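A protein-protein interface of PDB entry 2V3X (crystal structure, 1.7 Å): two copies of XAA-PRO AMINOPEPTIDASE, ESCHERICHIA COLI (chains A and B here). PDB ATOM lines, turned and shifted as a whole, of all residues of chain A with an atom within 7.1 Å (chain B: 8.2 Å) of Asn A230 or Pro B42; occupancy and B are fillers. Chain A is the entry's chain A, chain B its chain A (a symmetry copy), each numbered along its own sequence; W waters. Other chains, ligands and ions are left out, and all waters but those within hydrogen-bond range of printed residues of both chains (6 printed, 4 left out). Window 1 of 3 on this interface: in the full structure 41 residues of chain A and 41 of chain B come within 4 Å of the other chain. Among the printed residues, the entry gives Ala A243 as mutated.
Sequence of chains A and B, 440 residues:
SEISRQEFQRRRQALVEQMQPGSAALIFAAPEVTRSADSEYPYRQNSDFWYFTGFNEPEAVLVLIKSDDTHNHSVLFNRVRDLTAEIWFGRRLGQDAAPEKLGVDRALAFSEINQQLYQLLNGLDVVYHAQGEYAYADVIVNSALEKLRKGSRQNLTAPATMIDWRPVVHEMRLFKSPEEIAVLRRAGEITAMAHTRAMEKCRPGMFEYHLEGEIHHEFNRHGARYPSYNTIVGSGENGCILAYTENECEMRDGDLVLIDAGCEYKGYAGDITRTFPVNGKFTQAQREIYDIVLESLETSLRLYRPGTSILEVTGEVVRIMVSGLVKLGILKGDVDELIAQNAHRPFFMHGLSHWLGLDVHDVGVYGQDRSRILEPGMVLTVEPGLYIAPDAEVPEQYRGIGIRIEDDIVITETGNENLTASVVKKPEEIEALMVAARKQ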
ATOM      1  N   ARG A  35       7.581 -37.619  15.940  1.00  0.00           N
ATOM      2  CA  ARG A  35       7.023 -36.296  15.706  1.00  0.00           C
ATOM      3  C   ARG A  35       6.114 -36.336  14.481  1.00  0.00           C
ATOM      4  O   ARG A  35       4.949 -35.925  14.554  1.00  0.00           O
ATOM      5  CB  ARG A  35       8.124 -35.230  15.521  1.00  0.00           C
ATOM      6  CG  ARG A  35       7.550 -33.836  15.312  1.00  0.00           C
ATOM      7  CD  ARG A  35       8.540 -32.692  15.475  1.00  0.00           C
ATOM      8  NE  ARG A  35       7.851 -31.408  15.317  1.00  0.00           N
ATOM      9  CZ  ARG A  35       7.616 -30.809  14.152  1.00  0.00           C
ATOM     10  NH1 ARG A  35       8.049 -31.325  13.003  1.00  0.00           N
ATOM     11  NH2 ARG A  35       6.942 -29.674  14.129  1.00  0.00           N
ATOM     12  N   TYR A  41      10.976 -36.622  17.806  1.00  0.00           N
ATOM     13  CA  TYR A  41      11.260 -35.506  18.665  1.00  0.00           C
ATOM     14  C   TYR A  41      12.652 -35.707  19.264  1.00  0.00           C
ATOM     15  O   TYR A  41      13.108 -36.848  19.370  1.00  0.00           O
ATOM     16  CB  TYR A  41      10.248 -35.447  19.811  1.00  0.00           C
ATOM     17  CG  TYR A  41       8.911 -34.840  19.455  1.00  0.00           C
ATOM     18  CD1 TYR A  41       8.759 -33.476  19.300  1.00  0.00           C
ATOM     19  CD2 TYR A  41       7.782 -35.644  19.319  1.00  0.00           C
ATOM     20  CE1 TYR A  41       7.528 -32.910  18.981  1.00  0.00           C
ATOM     21  CE2 TYR A  41       6.535 -35.094  19.017  1.00  0.00           C
ATOM     22  CZ  TYR A  41       6.414 -33.731  18.849  1.00  0.00           C
ATOM     23  OH  TYR A  41       5.188 -33.189  18.578  1.00  0.00           O
ATOM     24  N   GLU A 212       9.440 -15.798  22.681  1.00  0.00           N
ATOM     25  CA  GLU A 212       9.825 -17.196  22.821  1.00  0.00           C
ATOM     26  C   GLU A 212      11.199 -17.427  22.153  1.00  0.00           C
ATOM     27  O   GLU A 212      12.083 -18.087  22.729  1.00  0.00           O
ATOM     28  CB  GLU A 212       8.724 -18.090  22.229  1.00  0.00           C
ATOM     29  CG  GLU A 212       9.119 -19.529  21.966  1.00  0.00           C
ATOM     30  CD  GLU A 212       8.018 -20.304  21.252  1.00  0.00           C
ATOM     31  OE1 GLU A 212       6.828 -19.943  21.398  1.00  0.00           O
ATOM     32  OE2 GLU A 212       8.348 -21.259  20.506  1.00  0.00           O
ATOM     33  N   HIS A 216      14.479 -18.823  24.096  1.00  0.00           N
ATOM     34  CA  HIS A 216      15.136 -20.072  23.735  1.00  0.00           C
ATOM     35  C   HIS A 216      16.602 -19.895  23.306  1.00  0.00           C
ATOM     36  O   HIS A 216      17.445 -20.764  23.600  1.00  0.00           O
ATOM     37  CB  HIS A 216      14.355 -20.798  22.664  1.00  0.00           C
ATOM     38  CG  HIS A 216      13.009 -21.250  23.114  1.00  0.00           C
ATOM     39  ND1 HIS A 216      12.118 -21.827  22.240  1.00  0.00           N
ATOM     40  CD2 HIS A 216      12.400 -21.221  24.319  1.00  0.00           C
ATOM     41  CE1 HIS A 216      11.015 -22.155  22.901  1.00  0.00           C
ATOM     42  NE2 HIS A 216      11.155 -21.786  24.158  1.00  0.00           N
ATOM     43  N   PRO A 227      13.920 -26.148  26.445  1.00  0.00           N
ATOM     44  CA  PRO A 227      13.105 -25.713  27.585  1.00  0.00           C
ATOM     45  C   PRO A 227      12.598 -26.897  28.412  1.00  0.00           C
ATOM     46  O   PRO A 227      12.475 -28.007  27.906  1.00  0.00           O
ATOM     47  CB  PRO A 227      11.924 -25.008  26.935  1.00  0.00           C
ATOM     48  CG  PRO A 227      12.279 -24.846  25.506  1.00  0.00           C
ATOM     49  CD  PRO A 227      13.246 -25.904  25.159  1.00  0.00           C
ATOM     50  N   SER A 228      12.267 -26.643  29.672  1.00  0.00           N
ATOM     51  CA  SER A 228      11.700 -27.687  30.525  1.00  0.00           C
ATOM     52  C   SER A 228      10.202 -27.916  30.343  1.00  0.00           C
ATOM     53  O   SER A 228       9.648 -28.923  30.833  1.00  0.00           O
ATOM     54  CB  SER A 228      12.017 -27.381  31.988  1.00  0.00           C
ATOM     55  OG  SER A 228      11.540 -26.103  32.366  1.00  0.00           O
ATOM     56  N   TYR A 229       9.554 -27.014  29.623  1.00  0.00           N
ATOM     57  CA  TYR A 229       8.141 -27.109  29.287  1.00  0.00           C
ATOM     58  C   TYR A 229       7.878 -26.133  28.170  1.00  0.00           C
ATOM     59  O   TYR A 229       8.704 -25.261  27.903  1.00  0.00           O
ATOM     60  CB  TYR A 229       7.242 -26.797  30.476  1.00  0.00           C
ATOM     61  CG  TYR A 229       7.514 -25.496  31.137  1.00  0.00           C
ATOM     62  CD1 TYR A 229       8.484 -25.401  32.116  1.00  0.00           C
ATOM     63  CD2 TYR A 229       6.835 -24.327  30.771  1.00  0.00           C
ATOM     64  CE1 TYR A 229       8.783 -24.204  32.717  1.00  0.00           C
ATOM     65  CE2 TYR A 229       7.105 -23.123  31.394  1.00  0.00           C
ATOM     66  CZ  TYR A 229       8.090 -23.059  32.367  1.00  0.00           C
ATOM     67  OH  TYR A 229       8.421 -21.873  33.007  1.00  0.00           O
ATOM     68  N   ASN A 230       6.738 -26.252  27.522  1.00  0.00           N
ATOM     69  CA  ASN A 230       6.454 -25.368  26.396  1.00  0.00           C
ATOM     70  C   ASN A 230       6.216 -23.935  26.883  1.00  0.00           C
ATOM     71  O   ASN A 230       5.342 -23.663  27.709  1.00  0.00           O
ATOM     72  CB  ASN A 230       5.264 -25.879  25.586  1.00  0.00           C
ATOM     73  CG  ASN A 230       5.507 -27.269  25.035  1.00  0.00           C
ATOM     74  OD1 ASN A 230       6.613 -27.579  24.595  1.00  0.00           O
ATOM     75  ND2 ASN A 230       4.491 -28.100  25.057  1.00  0.00           N
ATOM     76  N   THR A 231       7.001 -23.032  26.319  1.00  0.00           N
ATOM     77  CA  THR A 231       7.011 -21.615  26.707  1.00  0.00           C
ATOM     78  C   THR A 231       5.660 -20.945  26.446  1.00  0.00           C
ATOM     79  O   THR A 231       5.076 -21.107  25.359  1.00  0.00           O
ATOM     80  CB  THR A 231       8.119 -20.889  25.924  1.00  0.00           C
ATOM     81  OG1 THR A 231       9.386 -21.431  26.309  1.00  0.00           O
ATOM     82  CG2 THR A 231       8.104 -19.354  26.165  1.00  0.00           C
ATOM     83  N   ILE A 232       5.196 -20.197  27.445  1.00  0.00           N
ATOM     84  CA  ILE A 232       3.919 -19.459  27.431  1.00  0.00           C
ATOM     85  C   ILE A 232       4.247 -17.968  27.275  1.00  0.00           C
ATOM     86  O   ILE A 232       4.986 -17.405  28.085  1.00  0.00           O
ATOM     87  CB  ILE A 232       3.184 -19.694  28.783  1.00  0.00           C
ATOM     88  CG1 ILE A 232       2.777 -21.164  28.898  1.00  0.00           C
ATOM     89  CG2 ILE A 232       1.999 -18.752  28.965  1.00  0.00           C
ATOM     90  CD1 ILE A 232       2.657 -21.643  30.339  1.00  0.00           C
ATOM     91  N   VAL A 233       3.716 -17.343  26.219  1.00  0.00           N
ATOM     92  CA  VAL A 233       3.818 -15.887  26.018  1.00  0.00           C
ATOM     93  C   VAL A 233       2.418 -15.342  25.713  1.00  0.00           C
ATOM     94  O   VAL A 233       1.984 -15.290  24.555  1.00  0.00           O
ATOM     95  CB  VAL A 233       4.815 -15.505  24.897  1.00  0.00           C
ATOM     96  CG1 VAL A 233       4.952 -13.944  24.773  1.00  0.00           C
ATOM     97  CG2 VAL A 233       6.195 -16.157  25.109  1.00  0.00           C
ATOM     98  N   ALA A 243      -1.878 -21.878  30.592  1.00  0.00           N
ATOM     99  CA  ALA A 243      -0.794 -22.522  29.834  1.00  0.00           C
ATOM    100  C   ALA A 243      -1.000 -22.266  28.337  1.00  0.00           C
ATOM    101  O   ALA A 243      -0.942 -23.181  27.512  1.00  0.00           O
ATOM    102  CB  ALA A 243      -0.759 -24.033  30.143  1.00  0.00           C
ATOM    103  N   TYR A 244      -1.227 -21.000  28.000  1.00  0.00           N
ATOM    104  CA  TYR A 244      -1.352 -20.543  26.604  1.00  0.00           C
ATOM    105  C   TYR A 244      -0.024 -20.734  25.894  1.00  0.00           C
ATOM    106  O   TYR A 244       0.962 -20.108  26.269  1.00  0.00           O
ATOM    107  CB  TYR A 244      -1.693 -19.049  26.603  1.00  0.00           C
ATOM    108  CG  TYR A 244      -1.668 -18.370  25.243  1.00  0.00           C
ATOM    109  CD1 TYR A 244      -2.717 -18.503  24.359  1.00  0.00           C
ATOM    110  CD2 TYR A 244      -0.590 -17.584  24.861  1.00  0.00           C
ATOM    111  CE1 TYR A 244      -2.696 -17.892  23.118  1.00  0.00           C
ATOM    112  CE2 TYR A 244      -0.561 -16.956  23.641  1.00  0.00           C
ATOM    113  CZ  TYR A 244      -1.618 -17.102  22.764  1.00  0.00           C
ATOM    114  OH  TYR A 244      -1.565 -16.464  21.547  1.00  0.00           O
ATOM    115  N   THR A 245       0.008 -21.573  24.863  1.00  0.00           N
ATOM    116  CA  THR A 245       1.278 -21.801  24.161  1.00  0.00           C
ATOM    117  C   THR A 245       1.226 -21.501  22.666  1.00  0.00           C
ATOM    118  O   THR A 245       2.246 -21.669  21.983  1.00  0.00           O
ATOM    119  CB  THR A 245       1.761 -23.244  24.377  1.00  0.00           C
ATOM    120  OG1 THR A 245       0.777 -24.144  23.854  1.00  0.00           O
ATOM    121  CG2 THR A 245       2.007 -23.518  25.891  1.00  0.00           C
ATOM    122  N   ASN A 247       1.056 -18.610  21.237  1.00  0.00           N
ATOM    123  CA  ASN A 247       2.028 -17.519  21.075  1.00  0.00           C
ATOM    124  C   ASN A 247       1.996 -16.912  19.676  1.00  0.00           C
ATOM    125  O   ASN A 247       3.032 -16.585  19.107  1.00  0.00           O
ATOM    126  CB  ASN A 247       3.440 -18.011  21.422  1.00  0.00           C
ATOM    127  CG  ASN A 247       3.544 -18.574  22.845  1.00  0.00           C
ATOM    128  OD1 ASN A 247       2.634 -18.441  23.668  1.00  0.00           O
ATOM    129  ND2 ASN A 247       4.665 -19.256  23.121  1.00  0.00           N
ATOM    130  N   ASP A 260       5.789 -17.283  30.892  1.00  0.00           N
ATOM    131  CA  ASP A 260       6.113 -18.400  31.792  1.00  0.00           C
ATOM    132  C   ASP A 260       7.033 -19.314  30.988  1.00  0.00           C
ATOM    133  O   ASP A 260       6.630 -19.889  29.976  1.00  0.00           O
ATOM    134  CB  ASP A 260       4.827 -19.103  32.216  1.00  0.00           C
ATOM    135  CG  ASP A 260       5.021 -20.080  33.387  1.00  0.00           C
ATOM    136  OD1 ASP A 260       6.145 -20.514  33.641  1.00  0.00           O
ATOM    137  OD2 ASP A 260       4.020 -20.395  34.064  1.00  0.00           O
ATOM    138  N   ALA A 261       8.302 -19.345  31.373  1.00  0.00           N
ATOM    139  CA  ALA A 261       9.312 -20.073  30.616  1.00  0.00           C
ATOM    140  C   ALA A 261      10.411 -20.524  31.539  1.00  0.00           C
ATOM    141  O   ALA A 261      10.767 -19.839  32.503  1.00  0.00           O
ATOM    142  CB  ALA A 261       9.919 -19.193  29.490  1.00  0.00           C
ATOM    143  N   GLY A 262      10.962 -21.683  31.218  1.00  0.00           N
ATOM    144  CA  GLY A 262      12.026 -22.269  32.010  1.00  0.00           C
ATOM    145  C   GLY A 262      12.920 -23.165  31.182  1.00  0.00           C
ATOM    146  O   GLY A 262      12.475 -23.835  30.252  1.00  0.00           O
ATOM    147  N   PRO B  31      -2.146 -37.972  17.914  1.00  0.00           N
ATOM    148  CA  PRO B  31      -2.248 -37.865  19.370  1.00  0.00           C
ATOM    149  C   PRO B  31      -1.245 -36.862  19.938  1.00  0.00           C
ATOM    150  O   PRO B  31      -0.203 -36.608  19.323  1.00  0.00           O
ATOM    151  CB  PRO B  31      -1.912 -39.286  19.858  1.00  0.00           C
ATOM    152  CG  PRO B  31      -1.206 -39.943  18.746  1.00  0.00           C
ATOM    153  CD  PRO B  31      -1.555 -39.236  17.461  1.00  0.00           C
ATOM    154  N   GLU B  32      -1.583 -36.274  21.077  1.00  0.00           N
ATOM    155  CA  GLU B  32      -0.593 -35.559  21.884  1.00  0.00           C
ATOM    156  C   GLU B  32       0.441 -36.576  22.384  1.00  0.00           C
ATOM    157  O   GLU B  32       0.123 -37.757  22.566  1.00  0.00           O
ATOM    158  CB  GLU B  32      -1.277 -34.860  23.044  1.00  0.00           C
ATOM    159  CG  GLU B  32      -2.234 -33.778  22.593  1.00  0.00           C
ATOM    160  CD  GLU B  32      -2.771 -32.929  23.732  1.00  0.00           C
ATOM    161  OE1 GLU B  32      -3.794 -33.305  24.340  1.00  0.00           O
ATOM    162  OE2 GLU B  32      -2.169 -31.865  23.995  1.00  0.00           O
ATOM    163  N   VAL B  33       1.659 -36.105  22.616  1.00  0.00           N
ATOM    164  CA  VAL B  33       2.826 -36.956  22.901  1.00  0.00           C
ATOM    165  C   VAL B  33       3.491 -36.455  24.201  1.00  0.00           C
ATOM    166  O   VAL B  33       3.853 -35.300  24.300  1.00  0.00           O
ATOM    167  CB  VAL B  33       3.875 -36.857  21.743  1.00  0.00           C
ATOM    168  CG1 VAL B  33       5.109 -37.656  22.065  1.00  0.00           C
ATOM    169  CG2 VAL B  33       3.301 -37.334  20.438  1.00  0.00           C
ATOM    170  N   THR B  34       3.671 -37.358  25.162  1.00  0.00           N
ATOM    171  CA  THR B  34       4.373 -37.032  26.412  1.00  0.00           C
ATOM    172  C   THR B  34       5.849 -36.796  26.157  1.00  0.00           C
ATOM    173  O   THR B  34       6.507 -37.564  25.449  1.00  0.00           O
ATOM    174  CB  THR B  34       4.241 -38.208  27.385  1.00  0.00           C
ATOM    175  OG1 THR B  34       2.866 -38.341  27.768  1.00  0.00           O
ATOM    176  CG2 THR B  34       5.157 -38.032  28.631  1.00  0.00           C
ATOM    177  N   ARG B  35       6.388 -35.745  26.786  1.00  0.00           N
ATOM    178  CA  ARG B  35       7.821 -35.507  26.847  1.00  0.00           C
ATOM    179  C   ARG B  35       8.381 -36.090  28.141  1.00  0.00           C
ATOM    180  O   ARG B  35       9.334 -36.880  28.109  1.00  0.00           O
ATOM    181  CB  ARG B  35       8.162 -34.005  26.746  1.00  0.00           C
ATOM    182  CG  ARG B  35       9.661 -33.748  26.773  1.00  0.00           C
ATOM    183  CD  ARG B  35      10.093 -32.359  26.328  1.00  0.00           C
ATOM    184  NE  ARG B  35      11.555 -32.262  26.333  1.00  0.00           N
ATOM    185  CZ  ARG B  35      12.295 -31.963  27.398  1.00  0.00           C
ATOM    186  NH1 ARG B  35      11.738 -31.666  28.572  1.00  0.00           N
ATOM    187  NH2 ARG B  35      13.611 -31.953  27.294  1.00  0.00           N
ATOM    188  N   ASP B  38       3.947 -35.230  33.244  1.00  0.00           N
ATOM    189  CA  ASP B  38       2.737 -34.554  32.766  1.00  0.00           C
ATOM    190  C   ASP B  38       3.001 -33.483  31.703  1.00  0.00           C
ATOM    191  O   ASP B  38       2.065 -32.805  31.269  1.00  0.00           O
ATOM    192  CB  ASP B  38       1.900 -33.990  33.931  1.00  0.00           C
ATOM    193  CG  ASP B  38       2.586 -32.860  34.689  1.00  0.00           C
ATOM    194  OD1 ASP B  38       3.835 -32.885  34.782  1.00  0.00           O
ATOM    195  OD2 ASP B  38       1.865 -31.972  35.232  1.00  0.00           O
ATOM    196  N   SER B  39       4.245 -33.350  31.227  1.00  0.00           N
ATOM    197  CA  SER B  39       4.539 -32.351  30.211  1.00  0.00           C
ATOM    198  C   SER B  39       4.562 -33.004  28.833  1.00  0.00           C
ATOM    199  O   SER B  39       5.050 -34.120  28.692  1.00  0.00           O
ATOM    200  CB  SER B  39       5.845 -31.618  30.480  1.00  0.00           C
ATOM    201  OG  SER B  39       6.967 -32.478  30.341  1.00  0.00           O
ATOM    202  N   GLU B  40       4.002 -32.308  27.844  1.00  0.00           N
ATOM    203  CA  GLU B  40       3.930 -32.803  26.480  1.00  0.00           C
ATOM    204  C   GLU B  40       4.867 -32.035  25.552  1.00  0.00           C
ATOM    205  O   GLU B  40       5.243 -30.884  25.819  1.00  0.00           O
ATOM    206  CB  GLU B  40       2.489 -32.698  25.986  1.00  0.00           C
ATOM    207  CG  GLU B  40       1.514 -33.504  26.831  1.00  0.00           C
ATOM    208  CD  GLU B  40       0.063 -33.131  26.593  1.00  0.00           C
ATOM    209  OE1 GLU B  40      -0.225 -32.395  25.617  1.00  0.00           O
ATOM    210  OE2 GLU B  40      -0.779 -33.578  27.395  1.00  0.00           O
ATOM    211  N   TYR B  41       5.270 -32.682  24.469  1.00  0.00           N
ATOM    212  CA  TYR B  41       5.984 -32.019  23.413  1.00  0.00           C
ATOM    213  C   TYR B  41       5.026 -31.045  22.727  1.00  0.00           C
ATOM    214  O   TYR B  41       3.811 -31.256  22.773  1.00  0.00           O
ATOM    215  CB  TYR B  41       6.459 -33.036  22.373  1.00  0.00           C
ATOM    216  CG  TYR B  41       7.708 -33.800  22.747  1.00  0.00           C
ATOM    217  CD1 TYR B  41       8.955 -33.210  22.685  1.00  0.00           C
ATOM    218  CD2 TYR B  41       7.634 -35.139  23.120  1.00  0.00           C
ATOM    219  CE1 TYR B  41      10.112 -33.911  23.018  1.00  0.00           C
ATOM    220  CE2 TYR B  41       8.783 -35.864  23.442  1.00  0.00           C
ATOM    221  CZ  TYR B  41      10.015 -35.247  23.390  1.00  0.00           C
ATOM    222  OH  TYR B  41      11.144 -35.963  23.681  1.00  0.00           O
ATOM    223  N   PRO B  42       5.571 -30.003  22.085  1.00  0.00           N
ATOM    224  CA  PRO B  42       4.734 -29.108  21.287  1.00  0.00           C
ATOM    225  C   PRO B  42       4.014 -29.944  20.232  1.00  0.00           C
ATOM    226  O   PRO B  42       4.622 -30.814  19.593  1.00  0.00           O
ATOM    227  CB  PRO B  42       5.720 -28.171  20.595  1.00  0.00           C
ATOM    228  CG  PRO B  42       7.021 -28.388  21.236  1.00  0.00           C
ATOM    229  CD  PRO B  42       6.999 -29.652  22.013  1.00  0.00           C
ATOM    230  N   TYR B  43       2.742 -29.662  20.055  1.00  0.00           N
ATOM    231  CA  TYR B  43       1.895 -30.496  19.210  1.00  0.00           C
ATOM    232  C   TYR B  43       2.299 -30.382  17.753  1.00  0.00           C
ATOM    233  O   TYR B  43       2.548 -29.273  17.253  1.00  0.00           O
ATOM    234  CB  TYR B  43       0.425 -30.082  19.360  1.00  0.00           C
ATOM    235  CG  TYR B  43      -0.517 -31.003  18.642  1.00  0.00           C
ATOM    236  CD1 TYR B  43      -0.666 -32.325  19.041  1.00  0.00           C
ATOM    237  CD2 TYR B  43      -1.261 -30.569  17.544  1.00  0.00           C
ATOM    238  CE1 TYR B  43      -1.508 -33.195  18.346  1.00  0.00           C
ATOM    239  CE2 TYR B  43      -2.105 -31.407  16.885  1.00  0.00           C
ATOM    240  CZ  TYR B  43      -2.238 -32.718  17.273  1.00  0.00           C
ATOM    241  OH  TYR B  43      -3.092 -33.560  16.611  1.00  0.00           O
ATOM    242  N   ARG B  44       2.353 -31.532  17.084  1.00  0.00           N
ATOM    243  CA  ARG B  44       2.555 -31.595  15.631  1.00  0.00           C
ATOM    244  C   ARG B  44       1.422 -32.417  15.031  1.00  0.00           C
ATOM    245  O   ARG B  44       1.280 -33.616  15.330  1.00  0.00           O
ATOM    246  CB  ARG B  44       3.910 -32.214  15.310  1.00  0.00           C
ATOM    247  CG  ARG B  44       4.144 -32.506  13.811  1.00  0.00           C
ATOM    248  CD  ARG B  44       3.852 -31.318  12.867  1.00  0.00           C
ATOM    249  NE  ARG B  44       4.731 -31.450  11.695  1.00  0.00           N
ATOM    250  CZ  ARG B  44       4.576 -32.341  10.708  1.00  0.00           C
ATOM    251  NH1 ARG B  44       3.504 -33.107  10.648  1.00  0.00           N
ATOM    252  NH2 ARG B  44       5.472 -32.418   9.705  1.00  0.00           N
ATOM    253  N   GLN B  45       0.609 -31.746  14.208  1.00  0.00           N
ATOM    254  CA  GLN B  45      -0.522 -32.393  13.555  1.00  0.00           C
ATOM    255  C   GLN B  45      -0.012 -33.425  12.568  1.00  0.00           C
ATOM    256  O   GLN B  45       1.054 -33.260  11.963  1.00  0.00           O
ATOM    257  CB  GLN B  45      -1.392 -31.354  12.828  1.00  0.00           C
ATOM    258  CG  GLN B  45      -2.684 -31.896  12.250  1.00  0.00           C
ATOM    259  CD  GLN B  45      -3.491 -32.650  13.294  1.00  0.00           C
ATOM    260  OE1 GLN B  45      -3.308 -33.864  13.484  1.00  0.00           O
ATOM    261  NE2 GLN B  45      -4.396 -31.942  13.951  1.00  0.00           N
ATOM    262  N   ASN B  56      -5.133 -27.517  13.749  1.00  0.00           N
ATOM    263  CA  ASN B  56      -3.997 -27.914  14.581  1.00  0.00           C
ATOM    264  C   ASN B  56      -4.382 -28.400  15.983  1.00  0.00           C
ATOM    265  O   ASN B  56      -3.669 -28.119  16.951  1.00  0.00           O
ATOM    266  CB  ASN B  56      -3.003 -26.763  14.685  1.00  0.00           C
ATOM    267  CG  ASN B  56      -1.616 -27.217  15.116  1.00  0.00           C
ATOM    268  OD1 ASN B  56      -1.151 -28.265  14.697  1.00  0.00           O
ATOM    269  ND2 ASN B  56      -0.944 -26.406  15.966  1.00  0.00           N
ATOM    270  N   ARG B 225       8.289 -21.400  13.764  1.00  0.00           N
ATOM    271  CA  ARG B 225       8.569 -21.611  15.185  1.00  0.00           C
ATOM    272  C   ARG B 225       9.415 -22.839  15.463  1.00  0.00           C
ATOM    273  O   ARG B 225      10.222 -22.849  16.390  1.00  0.00           O
ATOM    274  CB  ARG B 225       7.279 -21.731  16.012  1.00  0.00           C
ATOM    275  CG  ARG B 225       6.641 -20.427  16.381  1.00  0.00           C
ATOM    276  CD  ARG B 225       5.325 -20.699  17.121  1.00  0.00           C
ATOM    277  NE  ARG B 225       5.477 -20.929  18.555  1.00  0.00           N
ATOM    278  CZ  ARG B 225       4.552 -21.501  19.339  1.00  0.00           C
ATOM    279  NH1 ARG B 225       3.417 -21.991  18.834  1.00  0.00           N
ATOM    280  NH2 ARG B 225       4.754 -21.596  20.640  1.00  0.00           N
ATOM    281  N   TYR B 226       9.195 -23.896  14.690  1.00  0.00           N
ATOM    282  CA  TYR B 226       9.836 -25.197  14.928  1.00  0.00           C
ATOM    283  C   TYR B 226      10.661 -25.623  13.717  1.00  0.00           C
ATOM    284  O   TYR B 226      10.281 -25.371  12.571  1.00  0.00           O
ATOM    285  CB  TYR B 226       8.783 -26.281  15.188  1.00  0.00           C
ATOM    286  CG  TYR B 226       7.859 -25.919  16.332  1.00  0.00           C
ATOM    287  CD1 TYR B 226       8.338 -25.792  17.602  1.00  0.00           C
ATOM    288  CD2 TYR B 226       6.528 -25.679  16.109  1.00  0.00           C
ATOM    289  CE1 TYR B 226       7.490 -25.432  18.655  1.00  0.00           C
ATOM    290  CE2 TYR B 226       5.680 -25.313  17.142  1.00  0.00           C
ATOM    291  CZ  TYR B 226       6.181 -25.192  18.402  1.00  0.00           C
ATOM    292  OH  TYR B 226       5.329 -24.816  19.442  1.00  0.00           O
HETATM  293  O   HOH W   1       2.564 -33.964  18.983  1.00  0.00           O
HETATM  294  O   HOH W   2       8.295 -29.559  26.357  1.00  0.00           O
HETATM  295  O   HOH W   3       8.914 -30.993  29.201  1.00  0.00           O
HETATM  296  O   HOH W   4       5.165 -28.678  16.323  1.00  0.00           O
HETATM  297  O   HOH W   5      10.427 -20.890  18.286  1.00  0.00           O
HETATM  298  O   HOH W   6       5.111 -22.858  23.361  1.00  0.00           O
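Among the printed residues, merely in contact across the chains: Asn A230 with Pro B42 (3.3 Å), Tyr A41 with Tyr B41 (3.4 Å), Arg A35 with Arg B44 (3.6 Å), Tyr A41 with Arg B44 (3.6 Å), Pro A227 with Arg B35 (3.8 Å) and Asn A230 with Tyr B41 (3.8 Å).
Water W6 lies within hydrogen-bond range of O of Thr A231 (2.7 Å), NH2 of Arg B225 (3.0 Å) and O of Thr A245 (3.4 Å). Water W3 lies within hydrogen-bond range of OG of Ser B39, O of Ser A228 and NH1 of Arg B35. Water W5 bridges the backbone carbonyl oxygen (O) of Arg B225 (2.7 Å) and the side-chain carboxylate (OE2) of Glu A212 (3.1 Å). Water W1 bridges OH of Tyr A41 (2.8 Å) and N of Arg B44 (3.1 Å). Water W4 bridges the backbone carbonyl oxygen of Tyr B43 and the guanidinium group of Arg A35. Water W2 bridges the side-chain amide oxygen of Asn A230 (3.1 Å) and the backbone carbonyl oxygen of Glu B40 (3.4 Å).
The side-chain carboxylate (OE1) of Glu B40 lies close to the side-chain carboxylate (OE2) of Glu B32. O of Thr A231 lies within hydrogen-bond range of ND2 of Asn A247 (2.9 Å). The guanidinium group (NH1) of Arg B225 lies close to the side-chain hydroxyl (OH) of Tyr B226 (3.5 Å). N of Val A233 sits at hydrogen-bond distance from OD1 of Asn A247 (3.0 Å). The side-chain hydroxyl (OH) of Tyr A244 lies close to the backbone NH (N) of Asn A247 (3.4 Å). OE1 of Glu A212 sits at hydrogen-bond distance from ND2 of Asn A247, at 2.8 Å.
Printed residues of chain B within 4 Å of Glu A212: Arg B225 (2.8 Å). Printed residues of chain B within 4 Å of Asn A230: Glu B40, Tyr B41 and Pro B42. Of the printed residues of chain A, Glu B40 touches Asn A230 (3.0 Å). Printed residues of chain A within 4 Å of Tyr B41: Tyr A41 (3.4 Å) and Asn A230 (3.8 Å). Pro B42 touches just these residues of chain A: Tyr A41 (2.6 Å) and Asn A230 (3.3 Å). Of the printed residues of chain A, Arg B44 touches Arg A35 (3.6 Å) and Tyr A41 (3.6 Å). Of the printed residues of chain A, Arg B225 touches Glu A212 (2.8 Å), Thr A245 (2.8 Å) and Asn A247 (3.4 Å). The nearest printed residue of chain B that does not touch Asn A230 is Tyr B43 (5.5 Å). The nearest printed residue of chain B that does not touch Thr A245 is Tyr B226 (5.1 Å).
O of Pro B42 lies within hydrogen-bond range of OH of Tyr A41 (2.6 Å). The backbone carbonyl oxygen of Glu B40 lies within hydrogen-bond range of the side-chain amide nitrogen of Asn A230. OE1 of Glu A212 lies within salt-bridge range of NH2 of Arg B225, at 2.8 Å. NH2 of Arg B225 is in hydrogen-bond range of O of Thr A245 (2.8 Å). The guanidinium group (NH2) of Arg B225 lies close to the side-chain amide nitrogen (ND2) of Asn A247, 3.4 Å away.
Along chain B the printed residues that touch a printed residue of chain A span positions 35 to 225. Among the printed residues, 11 pairs touch across the chains.
Tyr A41 touches its own counterpart, Tyr B41.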
